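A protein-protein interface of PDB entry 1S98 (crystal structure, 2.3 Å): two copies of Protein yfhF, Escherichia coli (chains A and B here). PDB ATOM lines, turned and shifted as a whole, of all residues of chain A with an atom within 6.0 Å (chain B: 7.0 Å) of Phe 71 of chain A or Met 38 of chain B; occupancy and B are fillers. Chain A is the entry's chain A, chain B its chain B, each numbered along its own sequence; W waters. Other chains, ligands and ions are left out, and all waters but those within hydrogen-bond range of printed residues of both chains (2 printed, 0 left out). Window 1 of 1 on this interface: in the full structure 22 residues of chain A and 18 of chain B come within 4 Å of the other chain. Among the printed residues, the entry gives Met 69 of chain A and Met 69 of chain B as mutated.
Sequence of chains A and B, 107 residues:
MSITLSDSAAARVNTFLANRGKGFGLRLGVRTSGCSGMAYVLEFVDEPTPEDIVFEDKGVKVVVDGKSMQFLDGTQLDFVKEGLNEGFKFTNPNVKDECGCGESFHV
The backbone carbonyl oxygen (O) of Ser 36 of chain A lies within hydrogen-bond range of the backbone NH (N) of Tyr 40 of chain B, 3.0 Å away. The backbone carbonyl oxygen (O) of Phe 71 of chain A sits close to the side-chain amide oxygen (OE1) of Gln 70 of chain B (3.1 Å). OG of Ser 68 of chain A sits at hydrogen-bond distance from O of Asn 94 of chain B (2.6 Å). N of Tyr 40 of chain A is in hydrogen-bond range of O of Ser 36 of chain B (3.1 Å). The backbone carbonyl oxygen of Gln 70 of chain A lies close to the side-chain amide oxygen of Gln 70 of chain B (3.2 Å). SD of Met 38 of chain B is in hydrogen-bond range of OH of Tyr 40 of chain A. N of Met 38 of chain A is in hydrogen-bond range of O of Met 38 of chain B, at 2.7 Å. The side-chain amide oxygen (OE1) of Gln 70 of chain B lies close to the backbone carbonyl oxygen (O) of Asp 73 of chain A. SD of Met 38 of chain A is in hydrogen-bond range of OH of Tyr 40 of chain B, at 3.5 Å.
The backbone carbonyl oxygen (O) of Asp 73 of chain A lies close to the side-chain amide oxygen (OD1) of Asn 92 of chain A, 3.2 Å away. The side-chain amide nitrogen of Asn 92 of chain B sits close to the side-chain amide nitrogen of Asn 94 of chain B, 2.7 Å away. The backbone carbonyl oxygen (O) of Arg 31 of chain B lies within hydrogen-bond range of the backbone NH (N) of Ala 39 of chain B. The side-chain hydroxyl (OH) of Tyr 40 of chain B is in hydrogen-bond range of the side-chain amide oxygen (OD1) of Asn 92 of chain B (3.0 Å). The backbone carbonyl oxygen of Phe 71 of chain B sits at hydrogen-bond distance from the side-chain amide nitrogen of Asn 94 of chain B. The backbone carbonyl oxygen of Phe 71 of chain B lies close to the side-chain amide oxygen of Asn 92 of chain B, at 2.9 Å.
Ser 36 of chain A touches Tyr 40 of chain B, and with the chains exchanged Tyr 40 of chain A touches Ser 36 of chain B. Met 38 of chain A touches its own counterpart, Met 38 of chain B. Met 38 of chain A touches Tyr 40 of chain B, and with the chains exchanged Tyr 40 of chain A touches Met 38 of chain B. Phe 71 of chain A touches Met 38 of chain B, but with the chains exchanged Met 38 of chain A does not touch Phe 71 of chain B (5.2 Å). Positions printed for both chains: 30, 36, 37, 38, 39, 40, 69, 70, 71, 72, 92 and 95.
Of the 17 printed residues of chain B, 11 touch a printed residue of chain A. Hydrophobic or aromatic side chains of chain B within 4 Å of the printed part of chain A: Met 38, Ala 39, Tyr 40, Phe 71 and Val 95. Among the printed residues, 26 pairs touch across the chains. Among the printed residues, no Asp or Glu carboxylate lies within 4 Å of a Lys or Arg side-chain nitrogen of the other chain.
Met 38 of chain B touches five residues of chain A. Of the printed residues of chain B, Val 95 of chain A touches Arg 31 (3.8 Å), Thr 32 (3.8 Å), Met 38 (3.7 Å) and Phe 71 (3.2 Å). Of the printed residues of chain A, Gln 70 of chain B touches Gln 70, Phe 71 and Asp 73. Of the printed residues of chain B, Ser 36 of chain A touches Ala 39 and Tyr 40.
Val 30 of chain A touches Val 95 of chain B. Ala 39 of chain B touches Ser 36 of chain A. Met 38 of chain B touches Gly 37 of chain A (O to CA, 3.2 Å). CG2 of Val 95 of chain B touches CG of Met 38 of chain A (3.8 Å). Tyr 40 of chain A touches Gly 37 of chain B. Phe 71 of chain A touches Met 38 of chain B. Phe 71 of chain A touches Phe 71 of chain B. Phe 71 of chain A touches Asn 94 of chain B. N of Thr 32 of chain B touches CG1 of Val 95 of chain A, at 3.8 Å. Val 95 of chain A touches Phe 71 of chain B (CG2 to CZ, 3.2 Å).
Water W2 bridges the backbone carbonyl oxygen (O) of Ser 36 of chain B (2.7 Å) and the backbone carbonyl oxygen (O) of Tyr 40 of chain A (3.0 Å). Water W1 lies within hydrogen-bond range of the side-chain amide oxygen of Asn 94 of chain B (2.8 Å), the backbone NH of Phe 71 of chain A (2.9 Å), the backbone carbonyl oxygen of Lys 67 of chain A (3.1 Å) and the backbone NH of Gln 70 of chain A (3.4 Å).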
ATOM      1  N   VAL A  30      16.640   1.244  27.344  1.00  0.00           N
ATOM      2  CA  VAL A  30      15.651   0.153  27.287  1.00  0.00           C
ATOM      3  C   VAL A  30      15.723  -0.633  28.576  1.00  0.00           C
ATOM      4  O   VAL A  30      16.788  -0.987  28.978  1.00  0.00           O
ATOM      5  CB  VAL A  30      15.743  -0.679  26.000  1.00  0.00           C
ATOM      6  CG1 VAL A  30      17.068  -1.223  25.928  1.00  0.00           C
ATOM      7  CG2 VAL A  30      14.699  -1.823  25.996  1.00  0.00           C
ATOM      8  N   SER A  36       7.995 -10.832  30.025  1.00  0.00           N
ATOM      9  CA  SER A  36       8.313 -10.941  28.590  1.00  0.00           C
ATOM     10  C   SER A  36       8.379  -9.643  27.704  1.00  0.00           C
ATOM     11  O   SER A  36       8.295  -9.690  26.503  1.00  0.00           O
ATOM     12  CB  SER A  36       7.392 -11.977  27.926  1.00  0.00           C
ATOM     13  OG  SER A  36       6.125 -11.485  27.963  1.00  0.00           O
ATOM     14  N   GLY A  37       8.529  -8.508  28.363  1.00  0.00           N
ATOM     15  CA  GLY A  37       8.461  -7.184  27.739  1.00  0.00           C
ATOM     16  C   GLY A  37       9.755  -6.386  27.959  1.00  0.00           C
ATOM     17  O   GLY A  37      10.575  -6.685  28.833  1.00  0.00           O
ATOM     18  N   MET A  38       9.894  -5.359  27.135  1.00  0.00           N
ATOM     19  CA  MET A  38      11.044  -4.486  27.098  1.00  0.00           C
ATOM     20  C   MET A  38      10.356  -3.142  26.949  1.00  0.00           C
ATOM     21  O   MET A  38       9.416  -3.012  26.233  1.00  0.00           O
ATOM     22  CB  MET A  38      11.817  -4.743  25.842  1.00  0.00           C
ATOM     23  CG  MET A  38      13.145  -5.467  25.860  1.00  0.00           C
ATOM     24  SD  MET A  38      13.673  -6.802  24.660  1.00  0.00           S
ATOM     25  CE  MET A  38      12.508  -7.087  23.817  1.00  0.00           C
ATOM     26  N   ALA A  39      10.858  -2.109  27.597  1.00  0.00           N
ATOM     27  CA  ALA A  39      10.231  -0.761  27.505  1.00  0.00           C
ATOM     28  C   ALA A  39      11.316   0.183  27.268  1.00  0.00           C
ATOM     29  O   ALA A  39      12.323   0.168  27.957  1.00  0.00           O
ATOM     30  CB  ALA A  39       9.452  -0.379  28.717  1.00  0.00           C
ATOM     31  N   TYR A  40      11.099   1.008  26.256  1.00  0.00           N
ATOM     32  CA  TYR A  40      11.911   2.179  26.036  1.00  0.00           C
ATOM     33  C   TYR A  40      11.885   3.169  27.245  1.00  0.00           C
ATOM     34  O   TYR A  40      10.860   3.397  27.857  1.00  0.00           O
ATOM     35  CB  TYR A  40      11.463   2.863  24.789  1.00  0.00           C
ATOM     36  CG  TYR A  40      11.757   2.101  23.523  1.00  0.00           C
ATOM     37  CD1 TYR A  40      13.013   2.014  23.085  1.00  0.00           C
ATOM     38  CD2 TYR A  40      10.767   1.505  22.766  1.00  0.00           C
ATOM     39  CE1 TYR A  40      13.339   1.361  21.980  1.00  0.00           C
ATOM     40  CE2 TYR A  40      11.055   0.834  21.596  1.00  0.00           C
ATOM     41  CZ  TYR A  40      12.359   0.737  21.191  1.00  0.00           C
ATOM     42  OH  TYR A  40      12.841   0.112  20.062  1.00  0.00           O
ATOM     43  N   LYS A  67      26.229  -0.525  27.091  1.00  0.00           N
ATOM     44  CA  LYS A  67      25.744  -1.906  27.015  1.00  0.00           C
ATOM     45  C   LYS A  67      24.357  -2.033  26.321  1.00  0.00           C
ATOM     46  O   LYS A  67      23.890  -3.093  26.146  1.00  0.00           O
ATOM     47  CB  LYS A  67      25.727  -2.502  28.389  1.00  0.00           C
ATOM     48  CG  LYS A  67      27.125  -2.491  29.130  1.00  0.00           C
ATOM     49  CD  LYS A  67      26.983  -3.063  30.587  1.00  0.00           C
ATOM     50  CE  LYS A  67      28.259  -2.965  31.460  1.00  0.00           C
ATOM     51  NZ  LYS A  67      28.263  -1.619  32.227  1.00  0.00           N
ATOM     52  N   SER A  68      23.722  -0.899  25.987  1.00  0.00           N
ATOM     53  CA  SER A  68      22.517  -0.922  25.209  1.00  0.00           C
ATOM     54  C   SER A  68      22.587  -0.292  23.801  1.00  0.00           C
ATOM     55  O   SER A  68      21.595  -0.267  23.154  1.00  0.00           O
ATOM     56  CB  SER A  68      21.343  -0.348  25.985  1.00  0.00           C
ATOM     57  OG  SER A  68      21.010  -1.101  27.091  1.00  0.00           O
ATOM     58  N   MET A  69      23.780   0.127  23.380  1.00  0.00           N
ATOM     59  CA  MET A  69      24.075   0.869  22.164  1.00  0.00           C
ATOM     60  C   MET A  69      23.661   0.023  20.982  1.00  0.00           C
ATOM     61  O   MET A  69      22.841   0.436  20.209  1.00  0.00           O
ATOM     62  CB  MET A  69      25.551   1.171  22.132  1.00  0.00           C
ATOM     63  CG  MET A  69      25.981   2.315  21.352  1.00  0.00           C
ATOM     64  SD  MET A  69      27.846   2.549  21.663  1.00  0.00           S
ATOM     65  CE  MET A  69      27.915   3.840  22.673  1.00  0.00           C
ATOM     66  N   GLN A  70      24.143  -1.213  20.899  1.00  0.00           N
ATOM     67  CA  GLN A  70      23.784  -2.104  19.805  1.00  0.00           C
ATOM     68  C   GLN A  70      22.280  -2.405  19.728  1.00  0.00           C
ATOM     69  O   GLN A  70      21.744  -2.350  18.676  1.00  0.00           O
ATOM     70  CB  GLN A  70      24.579  -3.418  19.821  1.00  0.00           C
ATOM     71  CG  GLN A  70      26.020  -3.213  20.170  1.00  0.00           C
ATOM     72  CD  GLN A  70      27.121  -3.786  19.282  1.00  0.00           C
ATOM     73  OE1 GLN A  70      27.635  -3.078  18.413  1.00  0.00           O
ATOM     74  NE2 GLN A  70      27.577  -4.950  19.599  1.00  0.00           N
ATOM     75  N   PHE A  71      21.631  -2.678  20.859  1.00  0.00           N
ATOM     76  CA  PHE A  71      20.206  -2.819  20.905  1.00  0.00           C
ATOM     77  C   PHE A  71      19.491  -1.645  20.272  1.00  0.00           C
ATOM     78  O   PHE A  71      18.584  -1.784  19.485  1.00  0.00           O
ATOM     79  CB  PHE A  71      19.764  -2.990  22.328  1.00  0.00           C
ATOM     80  CG  PHE A  71      18.341  -3.286  22.511  1.00  0.00           C
ATOM     81  CD1 PHE A  71      17.946  -4.585  22.872  1.00  0.00           C
ATOM     82  CD2 PHE A  71      17.370  -2.350  22.368  1.00  0.00           C
ATOM     83  CE1 PHE A  71      16.612  -4.904  23.048  1.00  0.00           C
ATOM     84  CE2 PHE A  71      15.999  -2.653  22.562  1.00  0.00           C
ATOM     85  CZ  PHE A  71      15.628  -3.897  22.900  1.00  0.00           C
ATOM     86  N   LEU A  72      19.899  -0.458  20.664  1.00  0.00           N
ATOM     87  CA  LEU A  72      19.132   0.698  20.364  1.00  0.00           C
ATOM     88  C   LEU A  72      19.503   1.245  19.016  1.00  0.00           C
ATOM     89  O   LEU A  72      18.809   2.029  18.511  1.00  0.00           O
ATOM     90  CB  LEU A  72      19.314   1.756  21.462  1.00  0.00           C
ATOM     91  CG  LEU A  72      18.606   1.416  22.733  1.00  0.00           C
ATOM     92  CD1 LEU A  72      18.953   2.240  23.939  1.00  0.00           C
ATOM     93  CD2 LEU A  72      17.118   1.448  22.613  1.00  0.00           C
ATOM     94  N   ASP A  73      20.606   0.814  18.436  1.00  0.00           N
ATOM     95  CA  ASP A  73      20.977   1.292  17.110  1.00  0.00           C
ATOM     96  C   ASP A  73      19.808   1.112  16.156  1.00  0.00           C
ATOM     97  O   ASP A  73      19.089   0.144  16.215  1.00  0.00           O
ATOM     98  CB  ASP A  73      22.199   0.553  16.603  1.00  0.00           C
ATOM     99  CG  ASP A  73      22.886   1.231  15.445  1.00  0.00           C
ATOM    100  OD1 ASP A  73      23.546   0.497  14.713  1.00  0.00           O
ATOM    101  OD2 ASP A  73      22.845   2.459  15.204  1.00  0.00           O
ATOM    102  N   GLY A  74      19.572   2.087  15.307  1.00  0.00           N
ATOM    103  CA  GLY A  74      18.392   2.052  14.479  1.00  0.00           C
ATOM    104  C   GLY A  74      17.057   2.638  14.996  1.00  0.00           C
ATOM    105  O   GLY A  74      16.130   2.775  14.275  1.00  0.00           O
ATOM    106  N   THR A  75      16.960   2.974  16.252  1.00  0.00           N
ATOM    107  CA  THR A  75      15.701   3.502  16.697  1.00  0.00           C
ATOM    108  C   THR A  75      15.627   4.972  16.283  1.00  0.00           C
ATOM    109  O   THR A  75      16.587   5.657  16.202  1.00  0.00           O
ATOM    110  CB  THR A  75      15.374   3.276  18.194  1.00  0.00           C
ATOM    111  OG1 THR A  75      16.378   3.745  19.013  1.00  0.00           O
ATOM    112  CG2 THR A  75      15.521   1.697  18.561  1.00  0.00           C
ATOM    113  N   ASN A  92      11.812   1.256  14.913  1.00  0.00           N
ATOM    114  CA  ASN A  92      13.006   0.553  14.562  1.00  0.00           C
ATOM    115  C   ASN A  92      12.621  -0.371  13.442  1.00  0.00           C
ATOM    116  O   ASN A  92      11.757  -1.195  13.622  1.00  0.00           O
ATOM    117  CB  ASN A  92      13.581  -0.265  15.727  1.00  0.00           C
ATOM    118  CG  ASN A  92      15.023  -0.740  15.436  1.00  0.00           C
ATOM    119  OD1 ASN A  92      15.906  -0.476  16.201  1.00  0.00           O
ATOM    120  ND2 ASN A  92      15.256  -1.361  14.301  1.00  0.00           N
ATOM    121  N   VAL A  95      12.165  -4.251  14.034  1.00  0.00           N
ATOM    122  CA  VAL A  95      11.302  -4.757  15.087  1.00  0.00           C
ATOM    123  C   VAL A  95       9.949  -4.678  14.501  1.00  0.00           C
ATOM    124  O   VAL A  95       9.395  -3.608  14.351  1.00  0.00           O
ATOM    125  CB  VAL A  95      11.432  -3.915  16.363  1.00  0.00           C
ATOM    126  CG1 VAL A  95      10.462  -4.264  17.421  1.00  0.00           C
ATOM    127  CG2 VAL A  95      12.843  -4.059  16.910  1.00  0.00           C
ATOM    128  N   VAL B  30      11.786 -10.998  18.580  1.00  0.00           N
ATOM    129  CA  VAL B  30      11.250  -9.787  19.156  1.00  0.00           C
ATOM    130  C   VAL B  30      10.177  -9.218  18.262  1.00  0.00           C
ATOM    131  O   VAL B  30      10.196  -9.355  17.103  1.00  0.00           O
ATOM    132  CB  VAL B  30      12.298  -8.755  19.369  1.00  0.00           C
ATOM    133  CG1 VAL B  30      13.314  -9.178  20.435  1.00  0.00           C
ATOM    134  CG2 VAL B  30      12.936  -8.429  18.124  1.00  0.00           C
ATOM    135  N   ARG B  31       9.224  -8.594  18.888  1.00  0.00           N
ATOM    136  CA  ARG B  31       8.230  -7.917  18.227  1.00  0.00           C
ATOM    137  C   ARG B  31       7.899  -6.625  18.972  1.00  0.00           C
ATOM    138  O   ARG B  31       8.215  -6.378  20.086  1.00  0.00           O
ATOM    139  CB  ARG B  31       6.989  -8.787  18.111  1.00  0.00           C
ATOM    140  CG  ARG B  31       6.210  -9.001  19.355  1.00  0.00           C
ATOM    141  CD  ARG B  31       4.978 -10.009  19.157  1.00  0.00           C
ATOM    142  NE  ARG B  31       4.426 -10.364  20.444  1.00  0.00           N
ATOM    143  CZ  ARG B  31       3.695  -9.567  21.194  1.00  0.00           C
ATOM    144  NH1 ARG B  31       3.362  -8.353  20.790  1.00  0.00           N
ATOM    145  NH2 ARG B  31       3.263  -9.967  22.354  1.00  0.00           N
ATOM    146  N   THR B  32       7.166  -5.841  18.282  1.00  0.00           N
ATOM    147  CA  THR B  32       6.610  -4.661  18.788  1.00  0.00           C
ATOM    148  C   THR B  32       5.538  -4.948  19.822  1.00  0.00           C
ATOM    149  O   THR B  32       4.812  -5.827  19.667  1.00  0.00           O
ATOM    150  CB  THR B  32       6.049  -3.923  17.578  1.00  0.00           C
ATOM    151  OG1 THR B  32       6.837  -2.777  17.346  1.00  0.00           O
ATOM    152  CG2 THR B  32       4.633  -3.528  17.798  1.00  0.00           C
ATOM    153  N   SER B  33       5.447  -4.104  20.848  1.00  0.00           N
ATOM    154  CA  SER B  33       4.413  -4.132  21.875  1.00  0.00           C
ATOM    155  C   SER B  33       3.921  -2.731  22.220  1.00  0.00           C
ATOM    156  O   SER B  33       4.349  -2.116  23.214  1.00  0.00           O
ATOM    157  CB  SER B  33       5.024  -4.789  23.113  1.00  0.00           C
ATOM    158  OG  SER B  33       4.098  -4.857  24.128  1.00  0.00           O
ATOM    159  N   GLY B  34       3.091  -2.175  21.361  1.00  0.00           N
ATOM    160  CA  GLY B  34       2.710  -0.752  21.423  1.00  0.00           C
ATOM    161  C   GLY B  34       3.855   0.150  20.984  1.00  0.00           C
ATOM    162  O   GLY B  34       4.898  -0.272  20.486  1.00  0.00           O
ATOM    163  N   SER B  36       5.692   2.274  22.657  1.00  0.00           N
ATOM    164  CA  SER B  36       6.709   2.489  23.671  1.00  0.00           C
ATOM    165  C   SER B  36       7.438   1.174  24.174  1.00  0.00           C
ATOM    166  O   SER B  36       8.192   1.191  25.207  1.00  0.00           O
ATOM    167  CB  SER B  36       6.093   3.262  24.840  1.00  0.00           C
ATOM    168  N   GLY B  37       7.226   0.053  23.486  1.00  0.00           N
ATOM    169  CA  GLY B  37       7.980  -1.131  23.863  1.00  0.00           C
ATOM    170  C   GLY B  37       7.965  -2.338  22.928  1.00  0.00           C
ATOM    171  O   GLY B  37       7.399  -2.276  21.873  1.00  0.00           O
ATOM    172  N   MET B  38       8.545  -3.441  23.411  1.00  0.00           N
ATOM    173  CA  MET B  38       8.792  -4.617  22.639  1.00  0.00           C
ATOM    174  C   MET B  38       8.510  -5.923  23.508  1.00  0.00           C
ATOM    175  O   MET B  38       8.615  -5.928  24.788  1.00  0.00           O
ATOM    176  CB  MET B  38      10.217  -4.621  22.097  1.00  0.00           C
ATOM    177  CG  MET B  38      10.625  -3.519  21.013  1.00  0.00           C
ATOM    178  SD  MET B  38      12.388  -3.301  20.773  1.00  0.00           S
ATOM    179  CE  MET B  38      12.928  -4.885  20.856  1.00  0.00           C
ATOM    180  N   ALA B  39       8.166  -7.013  22.835  1.00  0.00           N
ATOM    181  CA  ALA B  39       7.944  -8.268  23.518  1.00  0.00           C
ATOM    182  C   ALA B  39       8.800  -9.271  22.856  1.00  0.00           C
ATOM    183  O   ALA B  39       9.146  -9.117  21.710  1.00  0.00           O
ATOM    184  CB  ALA B  39       6.529  -8.676  23.504  1.00  0.00           C
ATOM    185  N   TYR B  40       9.197 -10.289  23.662  1.00  0.00           N
ATOM    186  CA  TYR B  40       9.918 -11.485  23.256  1.00  0.00           C
ATOM    187  C   TYR B  40       8.916 -12.380  22.426  1.00  0.00           C
ATOM    188  O   TYR B  40       7.763 -12.366  22.618  1.00  0.00           O
ATOM    189  CB  TYR B  40      10.528 -12.217  24.485  1.00  0.00           C
ATOM    190  CG  TYR B  40      11.729 -11.552  25.088  1.00  0.00           C
ATOM    191  CD1 TYR B  40      12.963 -11.578  24.483  1.00  0.00           C
ATOM    192  CD2 TYR B  40      11.637 -10.776  26.212  1.00  0.00           C
ATOM    193  CE1 TYR B  40      14.042 -10.829  24.942  1.00  0.00           C
ATOM    194  CE2 TYR B  40      12.768 -10.009  26.724  1.00  0.00           C
ATOM    195  CZ  TYR B  40      13.930 -10.038  26.107  1.00  0.00           C
ATOM    196  OH  TYR B  40      14.990  -9.357  26.613  1.00  0.00           O
ATOM    197  N   MET B  69      19.371 -10.157  16.061  1.00  0.00           N
ATOM    198  CA  MET B  69      20.515 -10.437  16.872  1.00  0.00           C
ATOM    199  C   MET B  69      20.944  -9.199  17.673  1.00  0.00           C
ATOM    200  O   MET B  69      21.373  -9.278  18.821  1.00  0.00           O
ATOM    201  CB  MET B  69      21.662 -10.971  16.038  1.00  0.00           C
ATOM    202  CG  MET B  69      21.607 -12.535  15.676  1.00  0.00           C
ATOM    203  SD  MET B  69      21.362 -13.663  17.024  1.00  0.00           S
ATOM    204  CE  MET B  69      22.622 -13.280  17.711  1.00  0.00           C
ATOM    205  N   GLN B  70      20.802  -8.032  17.051  1.00  0.00           N
ATOM    206  CA  GLN B  70      21.179  -6.790  17.714  1.00  0.00           C
ATOM    207  C   GLN B  70      20.347  -6.591  19.006  1.00  0.00           C
ATOM    208  O   GLN B  70      20.834  -5.927  19.978  1.00  0.00           O
ATOM    209  CB  GLN B  70      21.040  -5.569  16.756  1.00  0.00           C
ATOM    210  CG  GLN B  70      19.567  -5.029  16.602  1.00  0.00           C
ATOM    211  CD  GLN B  70      19.426  -3.664  15.915  1.00  0.00           C
ATOM    212  OE1 GLN B  70      19.354  -2.622  16.581  1.00  0.00           O
ATOM    213  NE2 GLN B  70      19.385  -3.677  14.634  1.00  0.00           N
ATOM    214  N   PHE B  71      19.103  -7.138  19.028  1.00  0.00           N
ATOM    215  CA  PHE B  71      18.296  -7.059  20.262  1.00  0.00           C
ATOM    216  C   PHE B  71      18.536  -8.178  21.363  1.00  0.00           C
ATOM    217  O   PHE B  71      18.228  -8.002  22.540  1.00  0.00           O
ATOM    218  CB  PHE B  71      16.800  -6.924  19.972  1.00  0.00           C
ATOM    219  CG  PHE B  71      16.500  -5.991  18.904  1.00  0.00           C
ATOM    220  CD1 PHE B  71      16.158  -6.452  17.661  1.00  0.00           C
ATOM    221  CD2 PHE B  71      16.578  -4.601  19.082  1.00  0.00           C
ATOM    222  CE1 PHE B  71      15.902  -5.558  16.616  1.00  0.00           C
ATOM    223  CE2 PHE B  71      16.335  -3.798  18.020  1.00  0.00           C
ATOM    224  CZ  PHE B  71      16.005  -4.307  16.801  1.00  0.00           C
ATOM    225  N   LEU B  72      19.140  -9.273  20.918  1.00  0.00           N
ATOM    226  CA  LEU B  72      18.997 -10.554  21.578  1.00  0.00           C
ATOM    227  C   LEU B  72      20.317 -11.132  22.017  1.00  0.00           C
ATOM    228  O   LEU B  72      20.338 -11.817  22.952  1.00  0.00           O
ATOM    229  CB  LEU B  72      18.245 -11.590  20.695  1.00  0.00           C
ATOM    230  CG  LEU B  72      16.817 -11.265  20.601  1.00  0.00           C
ATOM    231  CD1 LEU B  72      16.143 -12.079  19.444  1.00  0.00           C
ATOM    232  CD2 LEU B  72      16.146 -11.469  21.850  1.00  0.00           C
ATOM    233  N   ASN B  92      18.812 -10.790  29.447  1.00  0.00           N
ATOM    234  CA  ASN B  92      19.252 -10.099  28.289  1.00  0.00           C
ATOM    235  C   ASN B  92      20.173  -8.906  28.702  1.00  0.00           C
ATOM    236  O   ASN B  92      19.716  -7.945  29.222  1.00  0.00           O
ATOM    237  CB  ASN B  92      18.045  -9.693  27.410  1.00  0.00           C
ATOM    238  CG  ASN B  92      18.443  -9.004  26.113  1.00  0.00           C
ATOM    239  OD1 ASN B  92      17.566  -8.757  25.244  1.00  0.00           O
ATOM    240  ND2 ASN B  92      19.720  -8.726  25.946  1.00  0.00           N
ATOM    241  N   ASN B  94      21.644  -6.564  27.050  1.00  0.00           N
ATOM    242  CA  ASN B  94      21.357  -5.403  26.277  1.00  0.00           C
ATOM    243  C   ASN B  94      20.292  -4.541  26.902  1.00  0.00           C
ATOM    244  O   ASN B  94      20.101  -3.456  26.477  1.00  0.00           O
ATOM    245  CB  ASN B  94      20.822  -5.857  24.896  1.00  0.00           C
ATOM    246  CG  ASN B  94      21.792  -6.728  24.133  1.00  0.00           C
ATOM    247  OD1 ASN B  94      22.845  -6.298  23.727  1.00  0.00           O
ATOM    248  ND2 ASN B  94      21.404  -7.997  23.911  1.00  0.00           N
ATOM    249  N   VAL B  95      19.552  -5.094  27.844  1.00  0.00           N
ATOM    250  CA  VAL B  95      18.371  -4.548  28.461  1.00  0.00           C
ATOM    251  C   VAL B  95      18.662  -4.304  29.968  1.00  0.00           C
ATOM    252  O   VAL B  95      19.206  -5.180  30.615  1.00  0.00           O
ATOM    253  CB  VAL B  95      17.276  -5.574  28.417  1.00  0.00           C
ATOM    254  CG1 VAL B  95      16.156  -5.147  29.262  1.00  0.00           C
ATOM    255  CG2 VAL B  95      16.767  -5.748  26.983  1.00  0.00           C
HETATM  256  O   HOH W   1      23.219  -3.548  23.172  1.00  0.00           O
HETATM  257  O   HOH W   2       7.978   2.951  27.233  1.00  0.00           O
